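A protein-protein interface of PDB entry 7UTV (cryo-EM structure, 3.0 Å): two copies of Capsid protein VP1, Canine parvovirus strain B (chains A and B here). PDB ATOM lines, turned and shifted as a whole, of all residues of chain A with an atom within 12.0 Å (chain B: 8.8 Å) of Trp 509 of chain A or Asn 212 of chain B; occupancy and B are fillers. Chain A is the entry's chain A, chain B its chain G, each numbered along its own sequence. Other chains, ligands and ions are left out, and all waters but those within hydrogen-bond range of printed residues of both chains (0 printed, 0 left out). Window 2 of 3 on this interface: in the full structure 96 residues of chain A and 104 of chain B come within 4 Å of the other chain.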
ATOM      1  N   ARG A 504      -5.825   4.618  28.015  1.00  0.00           N
ATOM      2  CA  ARG A 504      -6.947   5.408  27.541  1.00  0.00           C
ATOM      3  C   ARG A 504      -7.961   4.531  26.812  1.00  0.00           C
ATOM      4  O   ARG A 504      -7.712   3.362  26.514  1.00  0.00           O
ATOM      5  CB  ARG A 504      -6.466   6.547  26.641  1.00  0.00           C
ATOM      6  CG  ARG A 504      -6.058   6.183  25.228  1.00  0.00           C
ATOM      7  CD  ARG A 504      -5.504   7.386  24.513  1.00  0.00           C
ATOM      8  NE  ARG A 504      -5.345   7.115  23.091  1.00  0.00           N
ATOM      9  CZ  ARG A 504      -6.285   7.239  22.165  1.00  0.00           C
ATOM     10  NH1 ARG A 504      -7.501   7.688  22.448  1.00  0.00           N
ATOM     11  NH2 ARG A 504      -6.001   6.904  20.911  1.00  0.00           N
ATOM     12  N   ALA A 505      -9.125   5.120  26.539  1.00  0.00           N
ATOM     13  CA  ALA A 505     -10.183   4.498  25.758  1.00  0.00           C
ATOM     14  C   ALA A 505     -10.688   5.499  24.730  1.00  0.00           C
ATOM     15  O   ALA A 505     -10.660   6.709  24.967  1.00  0.00           O
ATOM     16  CB  ALA A 505     -11.327   4.033  26.651  1.00  0.00           C
ATOM     17  N   SER A 506     -11.141   4.987  23.584  1.00  0.00           N
ATOM     18  CA  SER A 506     -11.563   5.810  22.449  1.00  0.00           C
ATOM     19  C   SER A 506     -13.061   6.083  22.536  1.00  0.00           C
ATOM     20  O   SER A 506     -13.891   5.388  21.947  1.00  0.00           O
ATOM     21  CB  SER A 506     -11.194   5.125  21.140  1.00  0.00           C
ATOM     22  OG  SER A 506     -11.465   3.734  21.201  1.00  0.00           O
ATOM     23  N   HIS A 507     -13.409   7.126  23.292  1.00  0.00           N
ATOM     24  CA  HIS A 507     -14.813   7.497  23.442  1.00  0.00           C
ATOM     25  C   HIS A 507     -15.353   8.216  22.215  1.00  0.00           C
ATOM     26  O   HIS A 507     -16.529   8.051  21.872  1.00  0.00           O
ATOM     27  CB  HIS A 507     -14.994   8.367  24.686  1.00  0.00           C
ATOM     28  CG  HIS A 507     -14.722   7.648  25.970  1.00  0.00           C
ATOM     29  ND1 HIS A 507     -14.526   8.306  27.165  1.00  0.00           N
ATOM     30  CD2 HIS A 507     -14.619   6.327  26.249  1.00  0.00           C
ATOM     31  CE1 HIS A 507     -14.311   7.421  28.123  1.00  0.00           C
ATOM     32  NE2 HIS A 507     -14.363   6.213  27.593  1.00  0.00           N
ATOM     33  N   THR A 508     -14.526   9.009  21.550  1.00  0.00           N
ATOM     34  CA  THR A 508     -14.968   9.768  20.397  1.00  0.00           C
ATOM     35  C   THR A 508     -14.897   8.933  19.132  1.00  0.00           C
ATOM     36  O   THR A 508     -14.159   7.950  19.046  1.00  0.00           O
ATOM     37  CB  THR A 508     -14.116  11.021  20.214  1.00  0.00           C
ATOM     38  OG1 THR A 508     -12.732  10.656  20.153  1.00  0.00           O
ATOM     39  CG2 THR A 508     -14.332  11.994  21.359  1.00  0.00           C
ATOM     40  N   TRP A 509     -15.687   9.338  18.146  1.00  0.00           N
ATOM     41  CA  TRP A 509     -15.529   8.816  16.798  1.00  0.00           C
ATOM     42  C   TRP A 509     -14.191   9.236  16.209  1.00  0.00           C
ATOM     43  O   TRP A 509     -13.470   8.411  15.642  1.00  0.00           O
ATOM     44  CB  TRP A 509     -16.691   9.307  15.944  1.00  0.00           C
ATOM     45  CG  TRP A 509     -16.634   9.032  14.482  1.00  0.00           C
ATOM     46  CD1 TRP A 509     -15.995   9.763  13.535  1.00  0.00           C
ATOM     47  CD2 TRP A 509     -17.306   7.987  13.783  1.00  0.00           C
ATOM     48  NE1 TRP A 509     -16.192   9.224  12.304  1.00  0.00           N
ATOM     49  CE2 TRP A 509     -17.003   8.131  12.429  1.00  0.00           C
ATOM     50  CE3 TRP A 509     -18.123   6.935  14.176  1.00  0.00           C
ATOM     51  CZ2 TRP A 509     -17.475   7.267  11.472  1.00  0.00           C
ATOM     52  CZ3 TRP A 509     -18.586   6.078  13.223  1.00  0.00           C
ATOM     53  CH2 TRP A 509     -18.266   6.249  11.888  1.00  0.00           C
ATOM     54  N   ASN A 510     -13.839  10.503  16.344  1.00  0.00           N
ATOM     55  CA  ASN A 510     -12.659  11.014  15.679  1.00  0.00           C
ATOM     56  C   ASN A 510     -11.387  10.572  16.405  1.00  0.00           C
ATOM     57  O   ASN A 510     -11.411  10.327  17.613  1.00  0.00           O
ATOM     58  CB  ASN A 510     -12.708  12.531  15.618  1.00  0.00           C
ATOM     59  CG  ASN A 510     -12.665  13.166  16.979  1.00  0.00           C
ATOM     60  OD1 ASN A 510     -13.697  13.343  17.621  1.00  0.00           O
ATOM     61  ND2 ASN A 510     -11.468  13.533  17.429  1.00  0.00           N
ATOM     62  N   PRO A 511     -10.260  10.473  15.704  1.00  0.00           N
ATOM     63  CA  PRO A 511      -8.992  10.211  16.384  1.00  0.00           C
ATOM     64  C   PRO A 511      -8.436  11.451  17.061  1.00  0.00           C
ATOM     65  O   PRO A 511      -8.827  12.581  16.765  1.00  0.00           O
ATOM     66  CB  PRO A 511      -8.082   9.761  15.245  1.00  0.00           C
ATOM     67  CG  PRO A 511      -8.592  10.419  14.113  1.00  0.00           C
ATOM     68  CD  PRO A 511     -10.055  10.506  14.251  1.00  0.00           C
ATOM     69  N   ILE A 512      -7.481  11.223  17.959  1.00  0.00           N
ATOM     70  CA  ILE A 512      -6.897  12.277  18.780  1.00  0.00           C
ATOM     71  C   ILE A 512      -5.540  12.710  18.237  1.00  0.00           C
ATOM     72  O   ILE A 512      -4.923  12.000  17.439  1.00  0.00           O
ATOM     73  CB  ILE A 512      -6.793  11.834  20.254  1.00  0.00           C
ATOM     74  CG1 ILE A 512      -5.968  10.547  20.439  1.00  0.00           C
ATOM     75  CG2 ILE A 512      -8.180  11.634  20.815  1.00  0.00           C
ATOM     76  CD1 ILE A 512      -5.368  10.410  21.824  1.00  0.00           C
ATOM     77  N   GLN A 513      -5.078  13.884  18.661  1.00  0.00           N
ATOM     78  CA  GLN A 513      -3.718  14.312  18.372  1.00  0.00           C
ATOM     79  C   GLN A 513      -2.740  13.336  19.003  1.00  0.00           C
ATOM     80  O   GLN A 513      -2.982  12.819  20.096  1.00  0.00           O
ATOM     81  CB  GLN A 513      -3.504  15.735  18.910  1.00  0.00           C
ATOM     82  CG  GLN A 513      -2.137  16.359  18.687  1.00  0.00           C
ATOM     83  CD  GLN A 513      -1.801  16.523  17.229  1.00  0.00           C
ATOM     84  OE1 GLN A 513      -1.127  15.684  16.635  1.00  0.00           O
ATOM     85  NE2 GLN A 513      -2.265  17.616  16.638  1.00  0.00           N
ATOM     86  N   GLN A 514      -1.639  13.066  18.304  1.00  0.00           N
ATOM     87  CA  GLN A 514      -0.650  12.096  18.753  1.00  0.00           C
ATOM     88  C   GLN A 514       0.743  12.572  18.374  1.00  0.00           C
ATOM     89  O   GLN A 514       0.924  13.310  17.403  1.00  0.00           O
ATOM     90  CB  GLN A 514      -0.878  10.713  18.140  1.00  0.00           C
ATOM     91  CG  GLN A 514      -2.141   9.992  18.554  1.00  0.00           C
ATOM     92  CD  GLN A 514      -2.039   9.378  19.910  1.00  0.00           C
ATOM     93  OE1 GLN A 514      -1.242   9.806  20.731  1.00  0.00           O
ATOM     94  NE2 GLN A 514      -2.840   8.359  20.162  1.00  0.00           N
ATOM     95  N   PRO A 544      -7.659  15.165  23.951  1.00  0.00           N
ATOM     96  CA  PRO A 544      -8.624  16.033  24.627  1.00  0.00           C
ATOM     97  C   PRO A 544      -9.510  15.263  25.589  1.00  0.00           C
ATOM     98  O   PRO A 544      -9.790  14.080  25.386  1.00  0.00           O
ATOM     99  CB  PRO A 544      -9.439  16.612  23.471  1.00  0.00           C
ATOM    100  CG  PRO A 544      -9.377  15.605  22.460  1.00  0.00           C
ATOM    101  CD  PRO A 544      -8.026  15.014  22.534  1.00  0.00           C
ATOM    102  N   LYS A 546     -13.110  15.730  28.349  1.00  0.00           N
ATOM    103  CA  LYS A 546     -14.407  16.376  28.474  1.00  0.00           C
ATOM    104  C   LYS A 546     -14.485  17.101  29.810  1.00  0.00           C
ATOM    105  O   LYS A 546     -14.504  16.466  30.867  1.00  0.00           O
ATOM    106  CB  LYS A 546     -15.470  15.295  28.340  1.00  0.00           C
ATOM    107  CG  LYS A 546     -16.903  15.733  28.345  1.00  0.00           C
ATOM    108  CD  LYS A 546     -17.801  14.516  28.170  1.00  0.00           C
ATOM    109  CE  LYS A 546     -18.061  13.798  29.479  1.00  0.00           C
ATOM    110  NZ  LYS A 546     -19.212  14.377  30.214  1.00  0.00           N
ATOM    111  N   TYR B  43     -26.104  13.228  11.681  1.00  0.00           N
ATOM    112  CA  TYR B  43     -25.439  14.213  12.517  1.00  0.00           C
ATOM    113  C   TYR B  43     -24.922  15.357  11.653  1.00  0.00           C
ATOM    114  O   TYR B  43     -24.294  15.121  10.620  1.00  0.00           O
ATOM    115  CB  TYR B  43     -24.273  13.566  13.259  1.00  0.00           C
ATOM    116  CG  TYR B  43     -24.645  12.678  14.417  1.00  0.00           C
ATOM    117  CD1 TYR B  43     -24.914  11.343  14.236  1.00  0.00           C
ATOM    118  CD2 TYR B  43     -24.697  13.173  15.697  1.00  0.00           C
ATOM    119  CE1 TYR B  43     -25.238  10.535  15.290  1.00  0.00           C
ATOM    120  CE2 TYR B  43     -25.020  12.373  16.752  1.00  0.00           C
ATOM    121  CZ  TYR B  43     -25.286  11.055  16.543  1.00  0.00           C
ATOM    122  OH  TYR B  43     -25.611  10.256  17.608  1.00  0.00           O
ATOM    123  N   TRP B  73     -31.142  13.163  17.929  1.00  0.00           N
ATOM    124  CA  TRP B  73     -31.702  12.656  19.171  1.00  0.00           C
ATOM    125  C   TRP B  73     -32.328  13.788  19.962  1.00  0.00           C
ATOM    126  O   TRP B  73     -32.025  14.965  19.746  1.00  0.00           O
ATOM    127  CB  TRP B  73     -30.632  12.000  20.044  1.00  0.00           C
ATOM    128  CG  TRP B  73     -30.093  10.737  19.526  1.00  0.00           C
ATOM    129  CD1 TRP B  73     -29.126  10.591  18.595  1.00  0.00           C
ATOM    130  CD2 TRP B  73     -30.468   9.422  19.926  1.00  0.00           C
ATOM    131  NE1 TRP B  73     -28.877   9.270  18.378  1.00  0.00           N
ATOM    132  CE2 TRP B  73     -29.690   8.529  19.190  1.00  0.00           C
ATOM    133  CE3 TRP B  73     -31.388   8.915  20.840  1.00  0.00           C
ATOM    134  CZ2 TRP B  73     -29.804   7.163  19.326  1.00  0.00           C
ATOM    135  CZ3 TRP B  73     -31.497   7.557  20.972  1.00  0.00           C
ATOM    136  CH2 TRP B  73     -30.714   6.698  20.218  1.00  0.00           C
ATOM    137  N   THR B 146     -20.614   9.503  29.573  1.00  0.00           N
ATOM    138  CA  THR B 146     -19.652   9.672  28.492  1.00  0.00           C
ATOM    139  C   THR B 146     -19.963  10.898  27.643  1.00  0.00           C
ATOM    140  O   THR B 146     -19.040  11.567  27.169  1.00  0.00           O
ATOM    141  CB  THR B 146     -19.626   8.428  27.610  1.00  0.00           C
ATOM    142  OG1 THR B 146     -20.925   8.209  27.056  1.00  0.00           O
ATOM    143  CG2 THR B 146     -19.207   7.198  28.403  1.00  0.00           C
ATOM    144  N   MET B 147     -21.238  11.213  27.441  1.00  0.00           N
ATOM    145  CA  MET B 147     -21.626  12.329  26.598  1.00  0.00           C
ATOM    146  C   MET B 147     -21.427  13.645  27.340  1.00  0.00           C
ATOM    147  O   MET B 147     -21.331  13.654  28.566  1.00  0.00           O
ATOM    148  CB  MET B 147     -23.085  12.202  26.188  1.00  0.00           C
ATOM    149  CG  MET B 147     -23.491  10.860  25.621  1.00  0.00           C
ATOM    150  SD  MET B 147     -22.526  10.333  24.208  1.00  0.00           S
ATOM    151  CE  MET B 147     -22.989  11.579  23.027  1.00  0.00           C
ATOM    152  N   TYR B 174     -24.674  19.577  21.230  1.00  0.00           N
ATOM    153  CA  TYR B 174     -23.567  19.927  22.109  1.00  0.00           C
ATOM    154  C   TYR B 174     -22.519  20.729  21.353  1.00  0.00           C
ATOM    155  O   TYR B 174     -22.415  20.660  20.128  1.00  0.00           O
ATOM    156  CB  TYR B 174     -22.938  18.684  22.731  1.00  0.00           C
ATOM    157  CG  TYR B 174     -22.117  17.847  21.803  1.00  0.00           C
ATOM    158  CD1 TYR B 174     -20.744  18.020  21.722  1.00  0.00           C
ATOM    159  CD2 TYR B 174     -22.693  16.866  21.034  1.00  0.00           C
ATOM    160  CE1 TYR B 174     -19.996  17.267  20.892  1.00  0.00           C
ATOM    161  CE2 TYR B 174     -21.947  16.099  20.211  1.00  0.00           C
ATOM    162  CZ  TYR B 174     -20.599  16.307  20.138  1.00  0.00           C
ATOM    163  OH  TYR B 174     -19.811  15.564  19.315  1.00  0.00           O
ATOM    164  N   VAL B 205     -10.849  18.420  18.627  1.00  0.00           N
ATOM    165  CA  VAL B 205     -12.000  17.824  17.962  1.00  0.00           C
ATOM    166  C   VAL B 205     -12.533  16.708  18.843  1.00  0.00           C
ATOM    167  O   VAL B 205     -11.781  15.819  19.262  1.00  0.00           O
ATOM    168  CB  VAL B 205     -11.611  17.310  16.572  1.00  0.00           C
ATOM    169  CG1 VAL B 205     -12.790  16.658  15.864  1.00  0.00           C
ATOM    170  CG2 VAL B 205     -11.079  18.430  15.696  1.00  0.00           C
ATOM    171  N   GLN B 206     -13.833  16.750  19.132  1.00  0.00           N
ATOM    172  CA  GLN B 206     -14.512  15.690  19.874  1.00  0.00           C
ATOM    173  C   GLN B 206     -15.894  15.503  19.266  1.00  0.00           C
ATOM    174  O   GLN B 206     -16.823  16.239  19.605  1.00  0.00           O
ATOM    175  CB  GLN B 206     -14.609  16.018  21.355  1.00  0.00           C
ATOM    176  CG  GLN B 206     -13.312  15.898  22.100  1.00  0.00           C
ATOM    177  CD  GLN B 206     -13.518  15.543  23.548  1.00  0.00           C
ATOM    178  OE1 GLN B 206     -14.363  16.121  24.226  1.00  0.00           O
ATOM    179  NE2 GLN B 206     -12.748  14.579  24.035  1.00  0.00           N
ATOM    180  N   PHE B 207     -16.018  14.523  18.378  1.00  0.00           N
ATOM    181  CA  PHE B 207     -17.284  14.162  17.754  1.00  0.00           C
ATOM    182  C   PHE B 207     -17.850  12.944  18.471  1.00  0.00           C
ATOM    183  O   PHE B 207     -17.325  11.835  18.326  1.00  0.00           O
ATOM    184  CB  PHE B 207     -17.059  13.893  16.265  1.00  0.00           C
ATOM    185  CG  PHE B 207     -18.253  13.356  15.529  1.00  0.00           C
ATOM    186  CD1 PHE B 207     -19.500  13.881  15.708  1.00  0.00           C
ATOM    187  CD2 PHE B 207     -18.098  12.353  14.605  1.00  0.00           C
ATOM    188  CE1 PHE B 207     -20.566  13.392  15.017  1.00  0.00           C
ATOM    189  CE2 PHE B 207     -19.167  11.861  13.913  1.00  0.00           C
ATOM    190  CZ  PHE B 207     -20.401  12.385  14.120  1.00  0.00           C
ATOM    191  N   TYR B 208     -18.919  13.153  19.234  1.00  0.00           N
ATOM    192  CA  TYR B 208     -19.588  12.114  20.000  1.00  0.00           C
ATOM    193  C   TYR B 208     -20.853  11.688  19.283  1.00  0.00           C
ATOM    194  O   TYR B 208     -21.493  12.497  18.607  1.00  0.00           O
ATOM    195  CB  TYR B 208     -19.980  12.599  21.383  1.00  0.00           C
ATOM    196  CG  TYR B 208     -18.851  12.912  22.296  1.00  0.00           C
ATOM    197  CD1 TYR B 208     -18.191  11.914  22.963  1.00  0.00           C
ATOM    198  CD2 TYR B 208     -18.473  14.213  22.529  1.00  0.00           C
ATOM    199  CE1 TYR B 208     -17.173  12.194  23.812  1.00  0.00           C
ATOM    200  CE2 TYR B 208     -17.460  14.505  23.376  1.00  0.00           C
ATOM    201  CZ  TYR B 208     -16.810  13.492  24.016  1.00  0.00           C
ATOM    202  OH  TYR B 208     -15.781  13.780  24.876  1.00  0.00           O
ATOM    203  N   THR B 209     -21.202  10.416  19.430  1.00  0.00           N
ATOM    204  CA  THR B 209     -22.429   9.862  18.886  1.00  0.00           C
ATOM    205  C   THR B 209     -23.067   8.959  19.923  1.00  0.00           C
ATOM    206  O   THR B 209     -22.371   8.243  20.645  1.00  0.00           O
ATOM    207  CB  THR B 209     -22.164   9.084  17.619  1.00  0.00           C
ATOM    208  OG1 THR B 209     -21.127   8.129  17.855  1.00  0.00           O
ATOM    209  CG2 THR B 209     -21.740  10.014  16.517  1.00  0.00           C
ATOM    210  N   ILE B 210     -24.395   9.018  20.004  1.00  0.00           N
ATOM    211  CA  ILE B 210     -25.125   8.181  20.949  1.00  0.00           C
ATOM    212  C   ILE B 210     -24.911   6.714  20.629  1.00  0.00           C
ATOM    213  O   ILE B 210     -24.816   5.876  21.532  1.00  0.00           O
ATOM    214  CB  ILE B 210     -26.621   8.542  20.942  1.00  0.00           C
ATOM    215  CG1 ILE B 210     -26.862   9.977  21.433  1.00  0.00           C
ATOM    216  CG2 ILE B 210     -27.418   7.558  21.768  1.00  0.00           C
ATOM    217  CD1 ILE B 210     -26.525  10.261  22.902  1.00  0.00           C
ATOM    218  N   GLU B 211     -24.840   6.377  19.344  1.00  0.00           N
ATOM    219  CA  GLU B 211     -24.837   4.976  18.950  1.00  0.00           C
ATOM    220  C   GLU B 211     -23.559   4.275  19.386  1.00  0.00           C
ATOM    221  O   GLU B 211     -23.604   3.127  19.841  1.00  0.00           O
ATOM    222  CB  GLU B 211     -25.044   4.862  17.446  1.00  0.00           C
ATOM    223  CG  GLU B 211     -26.446   5.254  16.968  1.00  0.00           C
ATOM    224  CD  GLU B 211     -26.653   6.748  16.842  1.00  0.00           C
ATOM    225  OE1 GLU B 211     -25.775   7.513  17.294  1.00  0.00           O
ATOM    226  OE2 GLU B 211     -27.697   7.163  16.295  1.00  0.00           O
ATOM    227  N   ASN B 212     -22.416   4.947  19.282  1.00  0.00           N
ATOM    228  CA  ASN B 212     -21.147   4.344  19.668  1.00  0.00           C
ATOM    229  C   ASN B 212     -20.843   4.463  21.152  1.00  0.00           C
ATOM    230  O   ASN B 212     -19.976   3.739  21.647  1.00  0.00           O
ATOM    231  CB  ASN B 212     -19.990   4.978  18.894  1.00  0.00           C
ATOM    232  CG  ASN B 212     -19.961   4.567  17.447  1.00  0.00           C
ATOM    233  OD1 ASN B 212     -19.282   3.615  17.077  1.00  0.00           O
ATOM    234  ND2 ASN B 212     -20.691   5.288  16.611  1.00  0.00           N
ATOM    235  N   SER B 213     -21.542   5.333  21.873  1.00  0.00           N
ATOM    236  CA  SER B 213     -21.208   5.627  23.256  1.00  0.00           C
ATOM    237  C   SER B 213     -21.953   4.761  24.255  1.00  0.00           C
ATOM    238  O   SER B 213     -21.358   4.365  25.265  1.00  0.00           O
ATOM    239  CB  SER B 213     -21.506   7.097  23.560  1.00  0.00           C
ATOM    240  OG  SER B 213     -20.777   7.959  22.704  1.00  0.00           O
ATOM    241  N   VAL B 214     -23.222   4.455  23.990  1.00  0.00           N
ATOM    242  CA  VAL B 214     -24.129   3.859  24.977  1.00  0.00           C
ATOM    243  C   VAL B 214     -24.955   2.772  24.311  1.00  0.00           C
ATOM    244  O   VAL B 214     -25.146   2.783  23.088  1.00  0.00           O
ATOM    245  CB  VAL B 214     -25.068   4.913  25.594  1.00  0.00           C
ATOM    246  CG1 VAL B 214     -24.293   5.844  26.506  1.00  0.00           C
ATOM    247  CG2 VAL B 214     -25.759   5.740  24.529  1.00  0.00           C
ATOM    248  N   PRO B 215     -25.451   1.801  25.087  1.00  0.00           N
ATOM    249  CA  PRO B 215     -26.438   0.880  24.516  1.00  0.00           C
ATOM    250  C   PRO B 215     -27.744   1.598  24.244  1.00  0.00           C
ATOM    251  O   PRO B 215     -28.122   2.520  24.967  1.00  0.00           O
ATOM    252  CB  PRO B 215     -26.607  -0.187  25.599  1.00  0.00           C
ATOM    253  CG  PRO B 215     -25.473  -0.043  26.467  1.00  0.00           C
ATOM    254  CD  PRO B 215     -25.125   1.387  26.462  1.00  0.00           C
ATOM    255  N   VAL B 216     -28.437   1.162  23.197  1.00  0.00           N
ATOM    256  CA  VAL B 216     -29.696   1.757  22.767  1.00  0.00           C
ATOM    257  C   VAL B 216     -30.756   0.671  22.821  1.00  0.00           C
ATOM    258  O   VAL B 216     -30.674  -0.319  22.084  1.00  0.00           O
ATOM    259  CB  VAL B 216     -29.584   2.356  21.358  1.00  0.00           C
ATOM    260  CG1 VAL B 216     -30.912   2.961  20.893  1.00  0.00           C
ATOM    261  CG2 VAL B 216     -28.457   3.392  21.299  1.00  0.00           C
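O of Asn 510 of chain A sits at hydrogen-bond distance from OG1 of Thr 508 of chain A (2.9 Å).
OG of Ser 213 of chain B lies within hydrogen-bond range of SD of Met 147 of chain B (3.3 Å).
OH of Tyr 174 of chain B lies within hydrogen-bond range of O of Gln 206 of chain B, at 3.1 Å.
The backbone NH of Tyr 208 of chain B lies within hydrogen-bond range of the side-chain hydroxyl of Tyr 174 of chain B (2.6 Å).
The side-chain amide oxygen of Gln 206 of chain B sits at hydrogen-bond distance from the side-chain hydroxyl of Tyr 208 of chain B (2.8 Å).
OG1 of Thr 209 of chain B sits at hydrogen-bond distance from ND2 of Asn 212 of chain B (3.1 Å).
No position is printed for both chains.
Among the printed residues, merely in contact across the chains: Lys 546 of chain A with Thr 146 of chain B, Asn 510 of chain A with Gln 206 of chain B, Thr 508 of chain A with Phe 207 of chain B, Thr 508 of chain A with Tyr 208 of chain B, Lys 546 of chain A with Tyr 208 of chain B, Trp 509 of chain A with Asn 212 of chain B and Thr 508 of chain A with Gln 206 of chain B.
Of the 17 printed residues of chain B, 7 touch a printed residue of chain A.
Printed residues of chain A that touch a printed residue of chain B: Thr 508, Trp 509, Asn 510, Pro 544 and Lys 546.
Hydrophobic or aromatic side chains of chain A within 4 Å of the printed part of chain B: Trp 509 and Pro 544.
Among the printed residues, 12 pairs touch across the chains.
Among the printed residues, no Asp or Glu carboxylate lies within 4 Å of a Lys or Arg side-chain nitrogen of the other chain.
The backbone NH (N) of Trp 509 of chain A sits at hydrogen-bond distance from the backbone carbonyl oxygen (O) of Phe 207 of chain B (3.0 Å).
ND2 of Asn 510 of chain A lies within hydrogen-bond range of O of Val 205 of chain B (2.9 Å).
The side-chain amide oxygen (OD1) of Asn 510 of chain A sits at hydrogen-bond distance from the backbone NH (N) of Phe 207 of chain B (2.7 Å).
The backbone carbonyl oxygen (O) of Pro 544 of chain A sits at hydrogen-bond distance from the side-chain amide nitrogen (NE2) of Gln 206 of chain B, 3.3 Å away.
O of Met 147 of chain B is in hydrogen-bond range of NZ of Lys 546 of chain A, at 2.8 Å.
Of the printed residues of chain B, Thr 508 of chain A touches Gln 206 (3.99 Å), Phe 207 (3.8 Å) and Tyr 208 (3.8 Å).
Of chain B, only Phe 207 (3.0 Å) and Asn 212 (3.9 Å) come within 4 Å of Trp 509 of chain A.
Of the printed residues of chain B, Pro 544 of chain A touches Gln 206 (3.3 Å).
Printed residues of chain B within 4 Å of Lys 546 of chain A: Thr 146, Met 147 and Tyr 208.
Tyr 43 of chain B touches none of the printed residues of chain A.
Of the printed residues of chain A, Met 147 of chain B touches Lys 546.
Phe 207 of chain B touches just these residues of chain A: Thr 508 (3.8 Å), Trp 509 (3.0 Å) and Asn 510 (2.7 Å).
Thr 209 of chain B touches none of the printed residues of chain A.
No residue of chain A comes within 4 Å of Ile 210 of chain B.
No residue of chain A comes within 4 Å of Glu 211 of chain B.
Asn 212 of chain B touches one residue of chain A.
The nearest residue of chain B that does not touch Trp 509 of chain A is Thr 209 of chain B (4.9 Å).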
